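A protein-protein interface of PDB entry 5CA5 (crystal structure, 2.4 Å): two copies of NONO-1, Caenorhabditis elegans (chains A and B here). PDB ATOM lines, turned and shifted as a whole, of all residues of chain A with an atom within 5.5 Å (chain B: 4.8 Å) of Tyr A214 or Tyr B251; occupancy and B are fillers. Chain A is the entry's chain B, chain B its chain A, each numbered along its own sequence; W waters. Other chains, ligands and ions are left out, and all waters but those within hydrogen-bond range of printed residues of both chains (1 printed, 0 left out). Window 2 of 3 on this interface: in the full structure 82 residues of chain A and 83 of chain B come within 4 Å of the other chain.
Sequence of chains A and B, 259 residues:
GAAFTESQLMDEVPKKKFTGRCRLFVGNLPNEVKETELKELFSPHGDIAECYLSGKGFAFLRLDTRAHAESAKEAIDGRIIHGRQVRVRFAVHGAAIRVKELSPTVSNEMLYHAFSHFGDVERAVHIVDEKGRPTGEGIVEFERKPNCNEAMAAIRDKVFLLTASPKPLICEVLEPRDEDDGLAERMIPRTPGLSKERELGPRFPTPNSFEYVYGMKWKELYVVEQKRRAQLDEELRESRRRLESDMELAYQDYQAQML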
ATOM      1  N   PHE A 210      33.082  10.166  -0.476  1.00  0.00           N
ATOM      2  CA  PHE A 210      31.646   9.875  -0.571  1.00  0.00           C
ATOM      3  C   PHE A 210      30.776  11.147  -0.644  1.00  0.00           C
ATOM      4  O   PHE A 210      29.864  11.229  -1.479  1.00  0.00           O
ATOM      5  CB  PHE A 210      31.229   8.971   0.611  1.00  0.00           C
ATOM      6  CG  PHE A 210      29.757   8.618   0.696  1.00  0.00           C
ATOM      7  CD1 PHE A 210      29.227   7.578  -0.069  1.00  0.00           C
ATOM      8  CD2 PHE A 210      28.911   9.298   1.569  1.00  0.00           C
ATOM      9  CE1 PHE A 210      27.871   7.239   0.030  1.00  0.00           C
ATOM     10  CE2 PHE A 210      27.563   8.959   1.661  1.00  0.00           C
ATOM     11  CZ  PHE A 210      27.052   7.929   0.898  1.00  0.00           C
ATOM     12  N   GLU A 211      31.062  12.140   0.214  1.00  0.00           N
ATOM     13  CA  GLU A 211      30.294  13.399   0.285  1.00  0.00           C
ATOM     14  C   GLU A 211      30.340  14.348  -0.953  1.00  0.00           C
ATOM     15  O   GLU A 211      29.455  15.199  -1.115  1.00  0.00           O
ATOM     16  CB  GLU A 211      30.642  14.165   1.552  1.00  0.00           C
ATOM     17  CG  GLU A 211      32.085  14.585   1.639  1.00  0.00           C
ATOM     18  CD  GLU A 211      32.390  15.554   2.758  1.00  0.00           C
ATOM     19  OE1 GLU A 211      31.447  15.961   3.486  1.00  0.00           O
ATOM     20  OE2 GLU A 211      33.575  15.954   2.855  1.00  0.00           O
ATOM     21  N   TYR A 212      31.380  14.218  -1.790  1.00  0.00           N
ATOM     22  CA  TYR A 212      31.594  15.027  -2.986  1.00  0.00           C
ATOM     23  C   TYR A 212      30.447  14.869  -3.979  1.00  0.00           C
ATOM     24  O   TYR A 212      30.047  15.851  -4.595  1.00  0.00           O
ATOM     25  CB  TYR A 212      32.957  14.671  -3.635  1.00  0.00           C
ATOM     26  CG  TYR A 212      33.283  15.418  -4.914  1.00  0.00           C
ATOM     27  CD1 TYR A 212      33.822  16.702  -4.878  1.00  0.00           C
ATOM     28  CD2 TYR A 212      33.001  14.861  -6.159  1.00  0.00           C
ATOM     29  CE1 TYR A 212      34.095  17.405  -6.055  1.00  0.00           C
ATOM     30  CE2 TYR A 212      33.293  15.542  -7.339  1.00  0.00           C
ATOM     31  CZ  TYR A 212      33.847  16.812  -7.284  1.00  0.00           C
ATOM     32  OH  TYR A 212      34.162  17.458  -8.461  1.00  0.00           O
ATOM     33  N   VAL A 213      29.946  13.634  -4.147  1.00  0.00           N
ATOM     34  CA  VAL A 213      28.867  13.304  -5.082  1.00  0.00           C
ATOM     35  C   VAL A 213      27.578  13.993  -4.618  1.00  0.00           C
ATOM     36  O   VAL A 213      26.835  14.527  -5.440  1.00  0.00           O
ATOM     37  CB  VAL A 213      28.751  11.757  -5.294  1.00  0.00           C
ATOM     38  CG1 VAL A 213      27.515  11.377  -6.099  1.00  0.00           C
ATOM     39  CG2 VAL A 213      29.992  11.216  -5.985  1.00  0.00           C
ATOM     40  N   TYR A 214      27.391  14.080  -3.295  1.00  0.00           N
ATOM     41  CA  TYR A 214      26.252  14.731  -2.678  1.00  0.00           C
ATOM     42  C   TYR A 214      26.355  16.280  -2.649  1.00  0.00           C
ATOM     43  O   TYR A 214      25.336  16.958  -2.662  1.00  0.00           O
ATOM     44  CB  TYR A 214      25.947  14.108  -1.305  1.00  0.00           C
ATOM     45  CG  TYR A 214      25.608  12.631  -1.378  1.00  0.00           C
ATOM     46  CD1 TYR A 214      24.320  12.202  -1.702  1.00  0.00           C
ATOM     47  CD2 TYR A 214      26.579  11.659  -1.149  1.00  0.00           C
ATOM     48  CE1 TYR A 214      24.001  10.845  -1.760  1.00  0.00           C
ATOM     49  CE2 TYR A 214      26.286  10.301  -1.259  1.00  0.00           C
ATOM     50  CZ  TYR A 214      24.989   9.895  -1.532  1.00  0.00           C
ATOM     51  OH  TYR A 214      24.712   8.547  -1.605  1.00  0.00           O
ATOM     52  N   GLY A 215      27.575  16.805  -2.636  1.00  0.00           N
ATOM     53  CA  GLY A 215      27.854  18.234  -2.707  1.00  0.00           C
ATOM     54  C   GLY A 215      27.733  18.749  -4.130  1.00  0.00           C
ATOM     55  O   GLY A 215      27.405  19.911  -4.347  1.00  0.00           O
ATOM     56  N   MET A 216      27.995  17.874  -5.115  1.00  0.00           N
ATOM     57  CA  MET A 216      27.847  18.193  -6.531  1.00  0.00           C
ATOM     58  C   MET A 216      26.364  18.178  -6.913  1.00  0.00           C
ATOM     59  O   MET A 216      25.954  18.934  -7.807  1.00  0.00           O
ATOM     60  CB  MET A 216      28.679  17.254  -7.414  1.00  0.00           C
ATOM     61  CG  MET A 216      30.189  17.581  -7.429  1.00  0.00           C
ATOM     62  SD  MET A 216      30.573  19.314  -7.749  1.00  0.00           S
ATOM     63  CE  MET A 216      30.669  19.303  -9.511  1.00  0.00           C
ATOM     64  N   LYS A 217      25.555  17.360  -6.196  1.00  0.00           N
ATOM     65  CA  LYS A 217      24.103  17.244  -6.393  1.00  0.00           C
ATOM     66  C   LYS A 217      23.439  18.510  -5.897  1.00  0.00           C
ATOM     67  O   LYS A 217      22.518  19.009  -6.531  1.00  0.00           O
ATOM     68  CB  LYS A 217      23.543  16.006  -5.665  1.00  0.00           C
ATOM     69  CG  LYS A 217      23.683  14.720  -6.462  1.00  0.00           C
ATOM     70  CD  LYS A 217      23.196  13.492  -5.711  1.00  0.00           C
ATOM     71  CE  LYS A 217      23.344  12.243  -6.552  1.00  0.00           C
ATOM     72  NZ  LYS A 217      24.097  11.181  -5.835  1.00  0.00           N
ATOM     73  N   TRP A 218      23.964  19.064  -4.803  1.00  0.00           N
ATOM     74  CA  TRP A 218      23.501  20.315  -4.231  1.00  0.00           C
ATOM     75  C   TRP A 218      23.819  21.525  -5.096  1.00  0.00           C
ATOM     76  O   TRP A 218      22.968  22.403  -5.237  1.00  0.00           O
ATOM     77  CB  TRP A 218      24.038  20.477  -2.819  1.00  0.00           C
ATOM     78  CG  TRP A 218      23.196  19.780  -1.796  1.00  0.00           C
ATOM     79  CD1 TRP A 218      23.543  18.691  -1.057  1.00  0.00           C
ATOM     80  CD2 TRP A 218      21.832  20.091  -1.445  1.00  0.00           C
ATOM     81  NE1 TRP A 218      22.513  18.343  -0.216  1.00  0.00           N
ATOM     82  CE2 TRP A 218      21.442  19.174  -0.447  1.00  0.00           C
ATOM     83  CE3 TRP A 218      20.916  21.091  -1.844  1.00  0.00           C
ATOM     84  CZ2 TRP A 218      20.173  19.216   0.151  1.00  0.00           C
ATOM     85  CZ3 TRP A 218      19.669  21.143  -1.232  1.00  0.00           C
ATOM     86  CH2 TRP A 218      19.305  20.210  -0.257  1.00  0.00           C
ATOM     87  N   ALA B 164      29.631  18.863   8.484  1.00  0.00           N
ATOM     88  CA  ALA B 164      29.560  17.458   8.011  1.00  0.00           C
ATOM     89  C   ALA B 164      28.575  17.335   6.826  1.00  0.00           C
ATOM     90  O   ALA B 164      28.615  16.366   6.046  1.00  0.00           O
ATOM     91  CB  ALA B 164      29.105  16.566   9.149  1.00  0.00           C
ATOM     92  N   PRO B 166      26.764  17.880   3.337  1.00  0.00           N
ATOM     93  CA  PRO B 166      27.238  18.058   1.956  1.00  0.00           C
ATOM     94  C   PRO B 166      26.701  19.307   1.219  1.00  0.00           C
ATOM     95  O   PRO B 166      26.996  19.484   0.047  1.00  0.00           O
ATOM     96  CB  PRO B 166      26.781  16.758   1.281  1.00  0.00           C
ATOM     97  CG  PRO B 166      25.557  16.358   2.006  1.00  0.00           C
ATOM     98  CD  PRO B 166      25.772  16.780   3.432  1.00  0.00           C
ATOM     99  N   MET B 247      19.556  11.666   0.686  1.00  0.00           N
ATOM    100  CA  MET B 247      20.890  11.822   1.249  1.00  0.00           C
ATOM    101  C   MET B 247      21.009  11.230   2.626  1.00  0.00           C
ATOM    102  O   MET B 247      21.954  10.505   2.861  1.00  0.00           O
ATOM    103  CB  MET B 247      21.331  13.278   1.224  1.00  0.00           C
ATOM    104  CG  MET B 247      21.497  13.762  -0.165  1.00  0.00           C
ATOM    105  SD  MET B 247      22.681  15.078  -0.296  1.00  0.00           S
ATOM    106  CE  MET B 247      22.533  15.441  -2.043  1.00  0.00           C
ATOM    107  N   GLU B 248      20.040  11.490   3.518  1.00  0.00           N
ATOM    108  CA  GLU B 248      19.960  10.949   4.880  1.00  0.00           C
ATOM    109  C   GLU B 248      19.935   9.428   4.842  1.00  0.00           C
ATOM    110  O   GLU B 248      20.647   8.792   5.613  1.00  0.00           O
ATOM    111  CB  GLU B 248      18.714  11.513   5.592  1.00  0.00           C
ATOM    112  CG  GLU B 248      18.466  10.994   7.002  1.00  0.00           C
ATOM    113  CD  GLU B 248      17.050  10.495   7.238  1.00  0.00           C
ATOM    114  OE1 GLU B 248      16.105  11.311   7.140  1.00  0.00           O
ATOM    115  OE2 GLU B 248      16.883   9.280   7.500  1.00  0.00           O
ATOM    116  N   LEU B 249      19.130   8.851   3.930  1.00  0.00           N
ATOM    117  CA  LEU B 249      19.010   7.404   3.771  1.00  0.00           C
ATOM    118  C   LEU B 249      20.303   6.749   3.285  1.00  0.00           C
ATOM    119  O   LEU B 249      20.686   5.706   3.818  1.00  0.00           O
ATOM    120  CB  LEU B 249      17.814   7.030   2.885  1.00  0.00           C
ATOM    121  CG  LEU B 249      16.441   7.145   3.569  1.00  0.00           C
ATOM    122  CD1 LEU B 249      15.331   7.419   2.551  1.00  0.00           C
ATOM    123  CD2 LEU B 249      16.140   5.923   4.450  1.00  0.00           C
ATOM    124  N   ALA B 250      20.980   7.376   2.304  1.00  0.00           N
ATOM    125  CA  ALA B 250      22.232   6.894   1.730  1.00  0.00           C
ATOM    126  C   ALA B 250      23.381   7.038   2.706  1.00  0.00           C
ATOM    127  O   ALA B 250      24.169   6.104   2.826  1.00  0.00           O
ATOM    128  CB  ALA B 250      22.537   7.620   0.442  1.00  0.00           C
ATOM    129  N   TYR B 251      23.465   8.175   3.427  1.00  0.00           N
ATOM    130  CA  TYR B 251      24.504   8.419   4.428  1.00  0.00           C
ATOM    131  C   TYR B 251      24.438   7.441   5.601  1.00  0.00           C
ATOM    132  O   TYR B 251      25.485   6.967   6.059  1.00  0.00           O
ATOM    133  CB  TYR B 251      24.398   9.837   4.952  1.00  0.00           C
ATOM    134  CG  TYR B 251      25.301  10.831   4.268  1.00  0.00           C
ATOM    135  CD1 TYR B 251      25.030  11.279   2.977  1.00  0.00           C
ATOM    136  CD2 TYR B 251      26.371  11.407   4.946  1.00  0.00           C
ATOM    137  CE1 TYR B 251      25.820  12.257   2.369  1.00  0.00           C
ATOM    138  CE2 TYR B 251      27.174  12.379   4.345  1.00  0.00           C
ATOM    139  CZ  TYR B 251      26.889  12.811   3.063  1.00  0.00           C
ATOM    140  OH  TYR B 251      27.688  13.786   2.522  1.00  0.00           O
ATOM    141  N   GLN B 252      23.212   7.120   6.062  1.00  0.00           N
ATOM    142  CA  GLN B 252      22.910   6.171   7.153  1.00  0.00           C
ATOM    143  C   GLN B 252      23.348   4.769   6.762  1.00  0.00           C
ATOM    144  O   GLN B 252      23.973   4.081   7.564  1.00  0.00           O
ATOM    145  CB  GLN B 252      21.391   6.198   7.465  1.00  0.00           C
ATOM    146  CG  GLN B 252      20.958   5.392   8.699  1.00  0.00           C
ATOM    147  CD  GLN B 252      19.496   5.533   9.058  1.00  0.00           C
ATOM    148  OE1 GLN B 252      18.706   6.211   8.379  1.00  0.00           O
ATOM    149  NE2 GLN B 252      19.106   4.887  10.148  1.00  0.00           N
ATOM    150  N   ASP B 253      23.034   4.357   5.522  1.00  0.00           N
ATOM    151  CA  ASP B 253      23.371   3.065   4.935  1.00  0.00           C
ATOM    152  C   ASP B 253      24.900   2.987   4.696  1.00  0.00           C
ATOM    153  O   ASP B 253      25.494   1.958   4.951  1.00  0.00           O
ATOM    154  CB  ASP B 253      22.574   2.906   3.632  1.00  0.00           C
ATOM    155  CG  ASP B 253      22.411   1.499   3.102  1.00  0.00           C
ATOM    156  OD1 ASP B 253      23.437   0.805   2.927  1.00  0.00           O
ATOM    157  OD2 ASP B 253      21.285   1.145   2.718  1.00  0.00           O
ATOM    158  N   TYR B 254      25.530   4.089   4.257  1.00  0.00           N
ATOM    159  CA  TYR B 254      26.973   4.167   4.054  1.00  0.00           C
ATOM    160  C   TYR B 254      27.707   4.089   5.367  1.00  0.00           C
ATOM    161  O   TYR B 254      28.682   3.342   5.473  1.00  0.00           O
ATOM    162  CB  TYR B 254      27.368   5.454   3.326  1.00  0.00           C
ATOM    163  CG  TYR B 254      28.859   5.591   3.083  1.00  0.00           C
ATOM    164  CD1 TYR B 254      29.509   4.792   2.141  1.00  0.00           C
ATOM    165  CD2 TYR B 254      29.612   6.548   3.764  1.00  0.00           C
ATOM    166  CE1 TYR B 254      30.873   4.940   1.885  1.00  0.00           C
ATOM    167  CE2 TYR B 254      30.982   6.695   3.524  1.00  0.00           C
ATOM    168  CZ  TYR B 254      31.603   5.898   2.575  1.00  0.00           C
ATOM    169  OH  TYR B 254      32.942   6.054   2.334  1.00  0.00           O
ATOM    170  N   GLN B 255      27.275   4.888   6.359  1.00  0.00           N
ATOM    171  CA  GLN B 255      27.941   4.846   7.646  1.00  0.00           C
ATOM    172  C   GLN B 255      27.800   3.493   8.349  1.00  0.00           C
ATOM    173  O   GLN B 255      28.691   3.106   9.109  1.00  0.00           O
ATOM    174  CB  GLN B 255      27.602   6.060   8.512  1.00  0.00           C
ATOM    175  CG  GLN B 255      28.326   7.360   8.056  1.00  0.00           C
ATOM    176  CD  GLN B 255      29.858   7.372   7.862  1.00  0.00           C
ATOM    177  OE1 GLN B 255      30.633   6.692   8.550  1.00  0.00           O
ATOM    178  NE2 GLN B 255      30.322   8.171   6.896  1.00  0.00           N
HETATM  179  O   HOH W   1      22.172  16.917   2.838  1.00  0.00           O
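SD of Met B247 sits at hydrogen-bond distance from NE1 of Trp A218, at 3.3 Å.
Phe A210 touches Ala B250.
Tyr B254 touches Phe A210 (CB to CZ, 3.5 Å).
OE1 of Glu A211 touches O of Ala B164, 3.8 Å away.
Pro B166 touches Glu A211.
Glu A211 touches Tyr B251 (CB to OH, 3.1 Å).
Met B247 touches Tyr A214.
OH of Tyr A214 touches CB of Ala B250 (3.1 Å).
Tyr B251 touches Tyr A214.
Pro B166 touches Gly A215 (O to CA, 3.1 Å).
Met B247 touches Lys A217 (CE to CB, 3.8 Å).
Of chain B, only Pro B166, Met B247, Ala B250 and Tyr B251 come within 4 Å of Tyr A214.
Of the printed residues of chain A, Tyr B254 touches Phe A210.
Printed residues of chain A within 4 Å of Ala B164: Glu A211 (3.8 Å).
Printed residues of chain A within 4 Å of Ala B250: Phe A210 and Tyr A214.
Of the printed residues of chain B, Gly A215 touches Pro B166.
Of the printed residues of chain B, Glu A211 touches Ala B164, Pro B166 and Tyr B251.
The nearest printed residue of chain B that does not touch Tyr A214 is Tyr B254 (6.4 Å).
The nearest printed residue of chain A that does not touch Tyr B251 is Tyr A212 (5.7 Å).
The nearest printed residue of chain A that does not touch Ala B250 is Lys A217 (7.4 Å).
Hydrophobic or aromatic side chains of chain B within 4 Å of the printed part of chain A: Pro B166, Met B247, Ala B250, Tyr B251 and Tyr B254.
Along chain B the printed residues that touch a printed residue of chain A span positions 164 to 254.
Hydrophobic or aromatic side chains of chain A within 4 Å of the printed part of chain B: Phe A210, Tyr A214 and Trp A218.
Among the printed residues, 14 pairs touch across the chains.
No position is printed for both chains.
Of the 14 pairs that touch across the chains among the printed residues, none has its exchanged pair printed and touching as well.
Water W1 bridges the indole nitrogen of Trp A218 (3.4 Å) and the side-chain sulfur of Met B247 (3.7 Å).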
